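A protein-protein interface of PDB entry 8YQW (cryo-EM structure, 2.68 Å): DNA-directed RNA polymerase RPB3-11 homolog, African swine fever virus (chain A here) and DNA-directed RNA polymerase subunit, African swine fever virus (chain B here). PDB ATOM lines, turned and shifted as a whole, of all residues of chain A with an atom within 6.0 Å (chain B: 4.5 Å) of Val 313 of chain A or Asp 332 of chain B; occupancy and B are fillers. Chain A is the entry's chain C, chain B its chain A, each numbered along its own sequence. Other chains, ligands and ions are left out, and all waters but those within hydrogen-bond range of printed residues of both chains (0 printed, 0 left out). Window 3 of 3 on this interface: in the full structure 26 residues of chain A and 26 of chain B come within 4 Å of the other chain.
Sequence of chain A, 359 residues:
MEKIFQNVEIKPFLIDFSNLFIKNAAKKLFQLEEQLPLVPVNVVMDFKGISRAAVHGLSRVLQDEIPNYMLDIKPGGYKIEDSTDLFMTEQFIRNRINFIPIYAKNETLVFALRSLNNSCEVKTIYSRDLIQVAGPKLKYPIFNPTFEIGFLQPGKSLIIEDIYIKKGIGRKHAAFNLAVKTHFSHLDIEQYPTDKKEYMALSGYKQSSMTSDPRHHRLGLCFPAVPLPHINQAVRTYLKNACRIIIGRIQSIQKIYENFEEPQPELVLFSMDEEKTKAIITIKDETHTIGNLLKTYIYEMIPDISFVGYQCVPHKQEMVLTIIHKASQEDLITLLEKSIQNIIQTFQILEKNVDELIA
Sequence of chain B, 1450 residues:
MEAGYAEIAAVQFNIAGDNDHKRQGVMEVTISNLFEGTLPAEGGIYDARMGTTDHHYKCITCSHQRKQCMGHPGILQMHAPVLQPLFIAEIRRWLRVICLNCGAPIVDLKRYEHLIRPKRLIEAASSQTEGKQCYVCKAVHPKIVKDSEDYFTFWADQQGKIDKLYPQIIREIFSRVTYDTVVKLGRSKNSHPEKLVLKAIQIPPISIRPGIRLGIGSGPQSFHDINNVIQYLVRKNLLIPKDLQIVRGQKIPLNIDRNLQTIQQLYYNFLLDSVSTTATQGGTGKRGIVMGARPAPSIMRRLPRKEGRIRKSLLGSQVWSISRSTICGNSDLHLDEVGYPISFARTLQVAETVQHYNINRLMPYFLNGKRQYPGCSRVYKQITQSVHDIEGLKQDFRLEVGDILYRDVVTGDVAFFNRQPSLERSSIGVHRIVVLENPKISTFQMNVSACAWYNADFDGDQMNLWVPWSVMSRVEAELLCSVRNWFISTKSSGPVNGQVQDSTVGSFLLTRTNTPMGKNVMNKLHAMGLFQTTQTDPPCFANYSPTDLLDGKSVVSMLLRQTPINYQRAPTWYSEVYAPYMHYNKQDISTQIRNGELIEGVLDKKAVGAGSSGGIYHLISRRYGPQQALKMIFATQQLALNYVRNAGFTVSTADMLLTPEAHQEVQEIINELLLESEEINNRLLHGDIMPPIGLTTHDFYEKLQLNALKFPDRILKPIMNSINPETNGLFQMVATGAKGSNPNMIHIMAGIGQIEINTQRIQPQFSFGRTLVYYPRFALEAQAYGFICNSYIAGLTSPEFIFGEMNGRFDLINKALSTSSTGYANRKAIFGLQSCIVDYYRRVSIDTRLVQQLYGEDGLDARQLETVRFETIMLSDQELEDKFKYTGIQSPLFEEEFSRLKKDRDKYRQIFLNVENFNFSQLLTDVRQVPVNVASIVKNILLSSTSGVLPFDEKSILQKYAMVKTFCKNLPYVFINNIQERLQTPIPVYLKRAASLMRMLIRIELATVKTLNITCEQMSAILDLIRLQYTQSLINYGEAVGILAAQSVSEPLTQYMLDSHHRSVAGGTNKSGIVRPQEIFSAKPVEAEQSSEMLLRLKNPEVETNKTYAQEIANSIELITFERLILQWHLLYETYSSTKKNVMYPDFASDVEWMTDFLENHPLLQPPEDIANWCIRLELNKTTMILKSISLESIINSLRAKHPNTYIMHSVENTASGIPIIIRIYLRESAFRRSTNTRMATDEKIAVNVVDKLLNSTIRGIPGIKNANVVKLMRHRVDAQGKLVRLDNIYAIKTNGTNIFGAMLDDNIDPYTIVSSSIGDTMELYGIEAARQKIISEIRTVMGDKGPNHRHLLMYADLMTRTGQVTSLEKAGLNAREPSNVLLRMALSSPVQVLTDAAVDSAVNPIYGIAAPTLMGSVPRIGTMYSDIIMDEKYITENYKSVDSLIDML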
ATOM      1  N   GLN A 311     -19.811  15.105   7.962  1.00  0.00           N
ATOM      2  CA  GLN A 311     -20.146  16.104   8.981  1.00  0.00           C
ATOM      3  C   GLN A 311     -18.937  16.875   9.510  1.00  0.00           C
ATOM      4  O   GLN A 311     -17.932  16.285   9.911  1.00  0.00           O
ATOM      5  CB  GLN A 311     -20.849  15.404  10.143  1.00  0.00           C
ATOM      6  CG  GLN A 311     -21.233  16.302  11.294  1.00  0.00           C
ATOM      7  CD  GLN A 311     -21.537  15.513  12.549  1.00  0.00           C
ATOM      8  OE1 GLN A 311     -21.034  14.407  12.735  1.00  0.00           O
ATOM      9  NE2 GLN A 311     -22.379  16.071  13.409  1.00  0.00           N
ATOM     10  N   CYS A 312     -19.045  18.206   9.495  1.00  0.00           N
ATOM     11  CA  CYS A 312     -18.047  19.115  10.056  1.00  0.00           C
ATOM     12  C   CYS A 312     -18.724  19.969  11.121  1.00  0.00           C
ATOM     13  O   CYS A 312     -19.467  20.898  10.793  1.00  0.00           O
ATOM     14  CB  CYS A 312     -17.426  20.004   8.978  1.00  0.00           C
ATOM     15  SG  CYS A 312     -16.672  19.138   7.595  1.00  0.00           S
ATOM     16  N   VAL A 313     -18.459  19.672  12.389  1.00  0.00           N
ATOM     17  CA  VAL A 313     -19.109  20.367  13.497  1.00  0.00           C
ATOM     18  C   VAL A 313     -18.308  21.614  13.854  1.00  0.00           C
ATOM     19  O   VAL A 313     -17.087  21.529  14.043  1.00  0.00           O
ATOM     20  CB  VAL A 313     -19.272  19.441  14.711  1.00  0.00           C
ATOM     21  CG1 VAL A 313     -19.770  20.217  15.902  1.00  0.00           C
ATOM     22  CG2 VAL A 313     -20.225  18.314  14.379  1.00  0.00           C
ATOM     23  N   PRO A 314     -18.944  22.789  13.934  1.00  0.00           N
ATOM     24  CA  PRO A 314     -18.175  24.019  14.196  1.00  0.00           C
ATOM     25  C   PRO A 314     -17.406  24.016  15.505  1.00  0.00           C
ATOM     26  O   PRO A 314     -16.302  24.569  15.561  1.00  0.00           O
ATOM     27  CB  PRO A 314     -19.259  25.106  14.179  1.00  0.00           C
ATOM     28  CG  PRO A 314     -20.342  24.545  13.338  1.00  0.00           C
ATOM     29  CD  PRO A 314     -20.354  23.075  13.630  1.00  0.00           C
ATOM     30  N   HIS A 315     -17.945  23.415  16.564  1.00  0.00           N
ATOM     31  CA  HIS A 315     -17.289  23.458  17.864  1.00  0.00           C
ATOM     32  C   HIS A 315     -16.300  22.321  18.072  1.00  0.00           C
ATOM     33  O   HIS A 315     -15.636  22.282  19.112  1.00  0.00           O
ATOM     34  CB  HIS A 315     -18.326  23.465  18.997  1.00  0.00           C
ATOM     35  CG  HIS A 315     -19.003  22.148  19.228  1.00  0.00           C
ATOM     36  ND1 HIS A 315     -18.410  21.116  19.922  1.00  0.00           N
ATOM     37  CD2 HIS A 315     -20.239  21.713  18.894  1.00  0.00           C
ATOM     38  CE1 HIS A 315     -19.242  20.093  19.981  1.00  0.00           C
ATOM     39  NE2 HIS A 315     -20.360  20.429  19.367  1.00  0.00           N
ATOM     40  N   LYS A 316     -16.181  21.400  17.117  1.00  0.00           N
ATOM     41  CA  LYS A 316     -15.186  20.343  17.195  1.00  0.00           C
ATOM     42  C   LYS A 316     -13.969  20.610  16.325  1.00  0.00           C
ATOM     43  O   LYS A 316     -12.894  20.075  16.614  1.00  0.00           O
ATOM     44  CB  LYS A 316     -15.804  18.997  16.801  1.00  0.00           C
ATOM     45  CG  LYS A 316     -16.900  18.532  17.738  1.00  0.00           C
ATOM     46  CD  LYS A 316     -17.359  17.128  17.405  1.00  0.00           C
ATOM     47  CE  LYS A 316     -16.413  16.092  17.984  1.00  0.00           C
ATOM     48  NZ  LYS A 316     -16.369  16.151  19.470  1.00  0.00           N
ATOM     49  N   GLN A 317     -14.120  21.413  15.271  1.00  0.00           N
ATOM     50  CA  GLN A 317     -12.999  21.885  14.459  1.00  0.00           C
ATOM     51  C   GLN A 317     -12.278  20.725  13.773  1.00  0.00           C
ATOM     52  O   GLN A 317     -11.058  20.581  13.860  1.00  0.00           O
ATOM     53  CB  GLN A 317     -12.033  22.716  15.305  1.00  0.00           C
ATOM     54  CG  GLN A 317     -12.662  23.980  15.862  1.00  0.00           C
ATOM     55  CD  GLN A 317     -11.738  24.737  16.790  1.00  0.00           C
ATOM     56  OE1 GLN A 317     -10.667  24.253  17.151  1.00  0.00           O
ATOM     57  NE2 GLN A 317     -12.148  25.937  17.179  1.00  0.00           N
ATOM     58  N   GLU A 318     -13.052  19.898  13.074  1.00  0.00           N
ATOM     59  CA  GLU A 318     -12.508  18.754  12.359  1.00  0.00           C
ATOM     60  C   GLU A 318     -13.551  18.247  11.375  1.00  0.00           C
ATOM     61  O   GLU A 318     -14.747  18.507  11.522  1.00  0.00           O
ATOM     62  CB  GLU A 318     -12.093  17.638  13.321  1.00  0.00           C
ATOM     63  CG  GLU A 318     -13.261  16.970  14.014  1.00  0.00           C
ATOM     64  CD  GLU A 318     -12.855  16.269  15.289  1.00  0.00           C
ATOM     65  OE1 GLU A 318     -11.686  16.417  15.702  1.00  0.00           O
ATOM     66  OE2 GLU A 318     -13.706  15.572  15.882  1.00  0.00           O
ATOM     67  N   ASN B 330     -26.759  25.981  20.361  1.00  0.00           N
ATOM     68  CA  ASN B 330     -25.841  25.068  19.686  1.00  0.00           C
ATOM     69  C   ASN B 330     -26.645  23.841  19.281  1.00  0.00           C
ATOM     70  O   ASN B 330     -27.050  23.057  20.143  1.00  0.00           O
ATOM     71  CB  ASN B 330     -24.675  24.699  20.594  1.00  0.00           C
ATOM     72  CG  ASN B 330     -23.561  23.976  19.860  1.00  0.00           C
ATOM     73  OD1 ASN B 330     -23.788  23.340  18.837  1.00  0.00           O
ATOM     74  ND2 ASN B 330     -22.348  24.083  20.379  1.00  0.00           N
ATOM     75  N   SER B 331     -26.878  23.680  17.983  1.00  0.00           N
ATOM     76  CA  SER B 331     -27.733  22.606  17.499  1.00  0.00           C
ATOM     77  C   SER B 331     -27.000  21.281  17.340  1.00  0.00           C
ATOM     78  O   SER B 331     -27.632  20.285  16.983  1.00  0.00           O
ATOM     79  CB  SER B 331     -28.380  23.011  16.172  1.00  0.00           C
ATOM     80  OG  SER B 331     -27.433  23.054  15.124  1.00  0.00           O
ATOM     81  N   ASP B 332     -25.694  21.241  17.594  1.00  0.00           N
ATOM     82  CA  ASP B 332     -24.943  19.995  17.545  1.00  0.00           C
ATOM     83  C   ASP B 332     -24.855  19.297  18.891  1.00  0.00           C
ATOM     84  O   ASP B 332     -24.321  18.187  18.959  1.00  0.00           O
ATOM     85  CB  ASP B 332     -23.529  20.243  17.019  1.00  0.00           C
ATOM     86  CG  ASP B 332     -23.509  20.603  15.555  1.00  0.00           C
ATOM     87  OD1 ASP B 332     -24.079  19.843  14.744  1.00  0.00           O
ATOM     88  OD2 ASP B 332     -22.914  21.641  15.212  1.00  0.00           O
ATOM     89  N   LEU B 333     -25.360  19.913  19.954  1.00  0.00           N
ATOM     90  CA  LEU B 333     -25.349  19.307  21.273  1.00  0.00           C
ATOM     91  C   LEU B 333     -26.635  18.530  21.502  1.00  0.00           C
ATOM     92  O   LEU B 333     -27.715  18.961  21.095  1.00  0.00           O
ATOM     93  CB  LEU B 333     -25.188  20.374  22.356  1.00  0.00           C
ATOM     94  CG  LEU B 333     -23.849  21.104  22.417  1.00  0.00           C
ATOM     95  CD1 LEU B 333     -23.942  22.265  23.375  1.00  0.00           C
ATOM     96  CD2 LEU B 333     -22.732  20.166  22.819  1.00  0.00           C
ATOM     97  N   HIS B 334     -26.511  17.376  22.150  1.00  0.00           N
ATOM     98  CA  HIS B 334     -27.683  16.620  22.548  1.00  0.00           C
ATOM     99  C   HIS B 334     -28.450  17.380  23.625  1.00  0.00           C
ATOM    100  O   HIS B 334     -27.964  18.352  24.205  1.00  0.00           O
ATOM    101  CB  HIS B 334     -27.284  15.236  23.052  1.00  0.00           C
ATOM    102  CG  HIS B 334     -26.742  14.337  21.986  1.00  0.00           C
ATOM    103  ND1 HIS B 334     -27.465  13.293  21.454  1.00  0.00           N
ATOM    104  CD2 HIS B 334     -25.545  14.326  21.355  1.00  0.00           C
ATOM    105  CE1 HIS B 334     -26.737  12.677  20.542  1.00  0.00           C
ATOM    106  NE2 HIS B 334     -25.569  13.284  20.461  1.00  0.00           N
ATOM    107  N   THR B 533     -25.652  14.118  10.131  1.00  0.00           N
ATOM    108  CA  THR B 533     -25.464  14.913  11.334  1.00  0.00           C
ATOM    109  C   THR B 533     -26.215  14.362  12.539  1.00  0.00           C
ATOM    110  O   THR B 533     -25.933  14.779  13.666  1.00  0.00           O
ATOM    111  CB  THR B 533     -25.901  16.366  11.074  1.00  0.00           C
ATOM    112  OG1 THR B 533     -25.316  16.817   9.848  1.00  0.00           O
ATOM    113  CG2 THR B 533     -25.428  17.294  12.175  1.00  0.00           C
ATOM    114  N   GLN B 535     -25.925  11.782  14.220  1.00  0.00           N
ATOM    115  CA  GLN B 535     -25.040  11.087  15.149  1.00  0.00           C
ATOM    116  C   GLN B 535     -25.568   9.722  15.572  1.00  0.00           C
ATOM    117  O   GLN B 535     -25.089   9.157  16.562  1.00  0.00           O
ATOM    118  CB  GLN B 535     -24.741  11.941  16.388  1.00  0.00           C
ATOM    119  CG  GLN B 535     -23.911  13.175  16.085  1.00  0.00           C
ATOM    120  CD  GLN B 535     -23.724  14.061  17.294  1.00  0.00           C
ATOM    121  OE1 GLN B 535     -24.042  13.674  18.416  1.00  0.00           O
ATOM    122  NE2 GLN B 535     -23.209  15.264  17.070  1.00  0.00           N
ATOM    123  N   PHE B 634     -33.337  14.847  19.323  1.00  0.00           N
ATOM    124  CA  PHE B 634     -32.137  15.339  18.657  1.00  0.00           C
ATOM    125  C   PHE B 634     -32.048  14.818  17.230  1.00  0.00           C
ATOM    126  O   PHE B 634     -31.763  15.576  16.298  1.00  0.00           O
ATOM    127  CB  PHE B 634     -30.897  14.938  19.459  1.00  0.00           C
ATOM    128  CG  PHE B 634     -29.601  15.339  18.818  1.00  0.00           C
ATOM    129  CD1 PHE B 634     -29.065  16.592  19.034  1.00  0.00           C
ATOM    130  CD2 PHE B 634     -28.915  14.457  18.004  1.00  0.00           C
ATOM    131  CE1 PHE B 634     -27.880  16.957  18.449  1.00  0.00           C
ATOM    132  CE2 PHE B 634     -27.731  14.822  17.416  1.00  0.00           C
ATOM    133  CZ  PHE B 634     -27.213  16.072  17.640  1.00  0.00           C
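Of chain B, only Asp 332 comes within 4 Å of Val 313 of chain A. Asp 332 of chain B touches just these residues of chain A: Val 313 (3.5 Å), Pro 314 (3.3 Å) and His 315 (3.9 Å). Of the printed residues of chain B, Gln 311 of chain A touches Thr 533 and Gln 535. Printed residues of chain A within 4 Å of Gln 535 of chain B: Gln 311 (3.8 Å). Of the printed residues of chain B, His 315 of chain A touches Asn 330 (3.5 Å) and Asp 332 (3.9 Å). Printed residues of chain A within 4 Å of Thr 533 of chain B: Gln 311 (3.5 Å). Printed residues of chain B within 4 Å of Pro 314 of chain A: Asp 332 (3.3 Å). Phe 634 of chain B touches none of the printed residues of chain A. Ser 331 of chain B touches none of the printed residues of chain A. The nearest residue of chain A that does not touch Asp 332 of chain B is Gln 311 of chain A (4.3 Å).
Hydrophobic or aromatic side chains of chain A within 4 Å of the printed part of chain B: Val 313, Pro 314 and His 315. Among the printed residues, 6 pairs touch across the chains. Among the printed residues, no Asp or Glu carboxylate lies within 4 Å of a Lys or Arg side-chain nitrogen of the other chain.
The backbone NH of Asp 332 of chain B is in hydrogen-bond range of the side-chain amide oxygen of Asn 330 of chain B. OE1 of Gln 535 of chain B sits at hydrogen-bond distance from NE2 of His 334 of chain B, at 2.6 Å.
Among the printed residues, merely in contact across the chains: Pro 314 of chain A with Asp 332 of chain B, His 315 of chain A with Asn 330 of chain B, Gln 311 of chain A with Thr 533 of chain B, Val 313 of chain A with Asp 332 of chain B, Gln 311 of chain A with Gln 535 of chain B and His 315 of chain A with Asp 332 of chain B.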
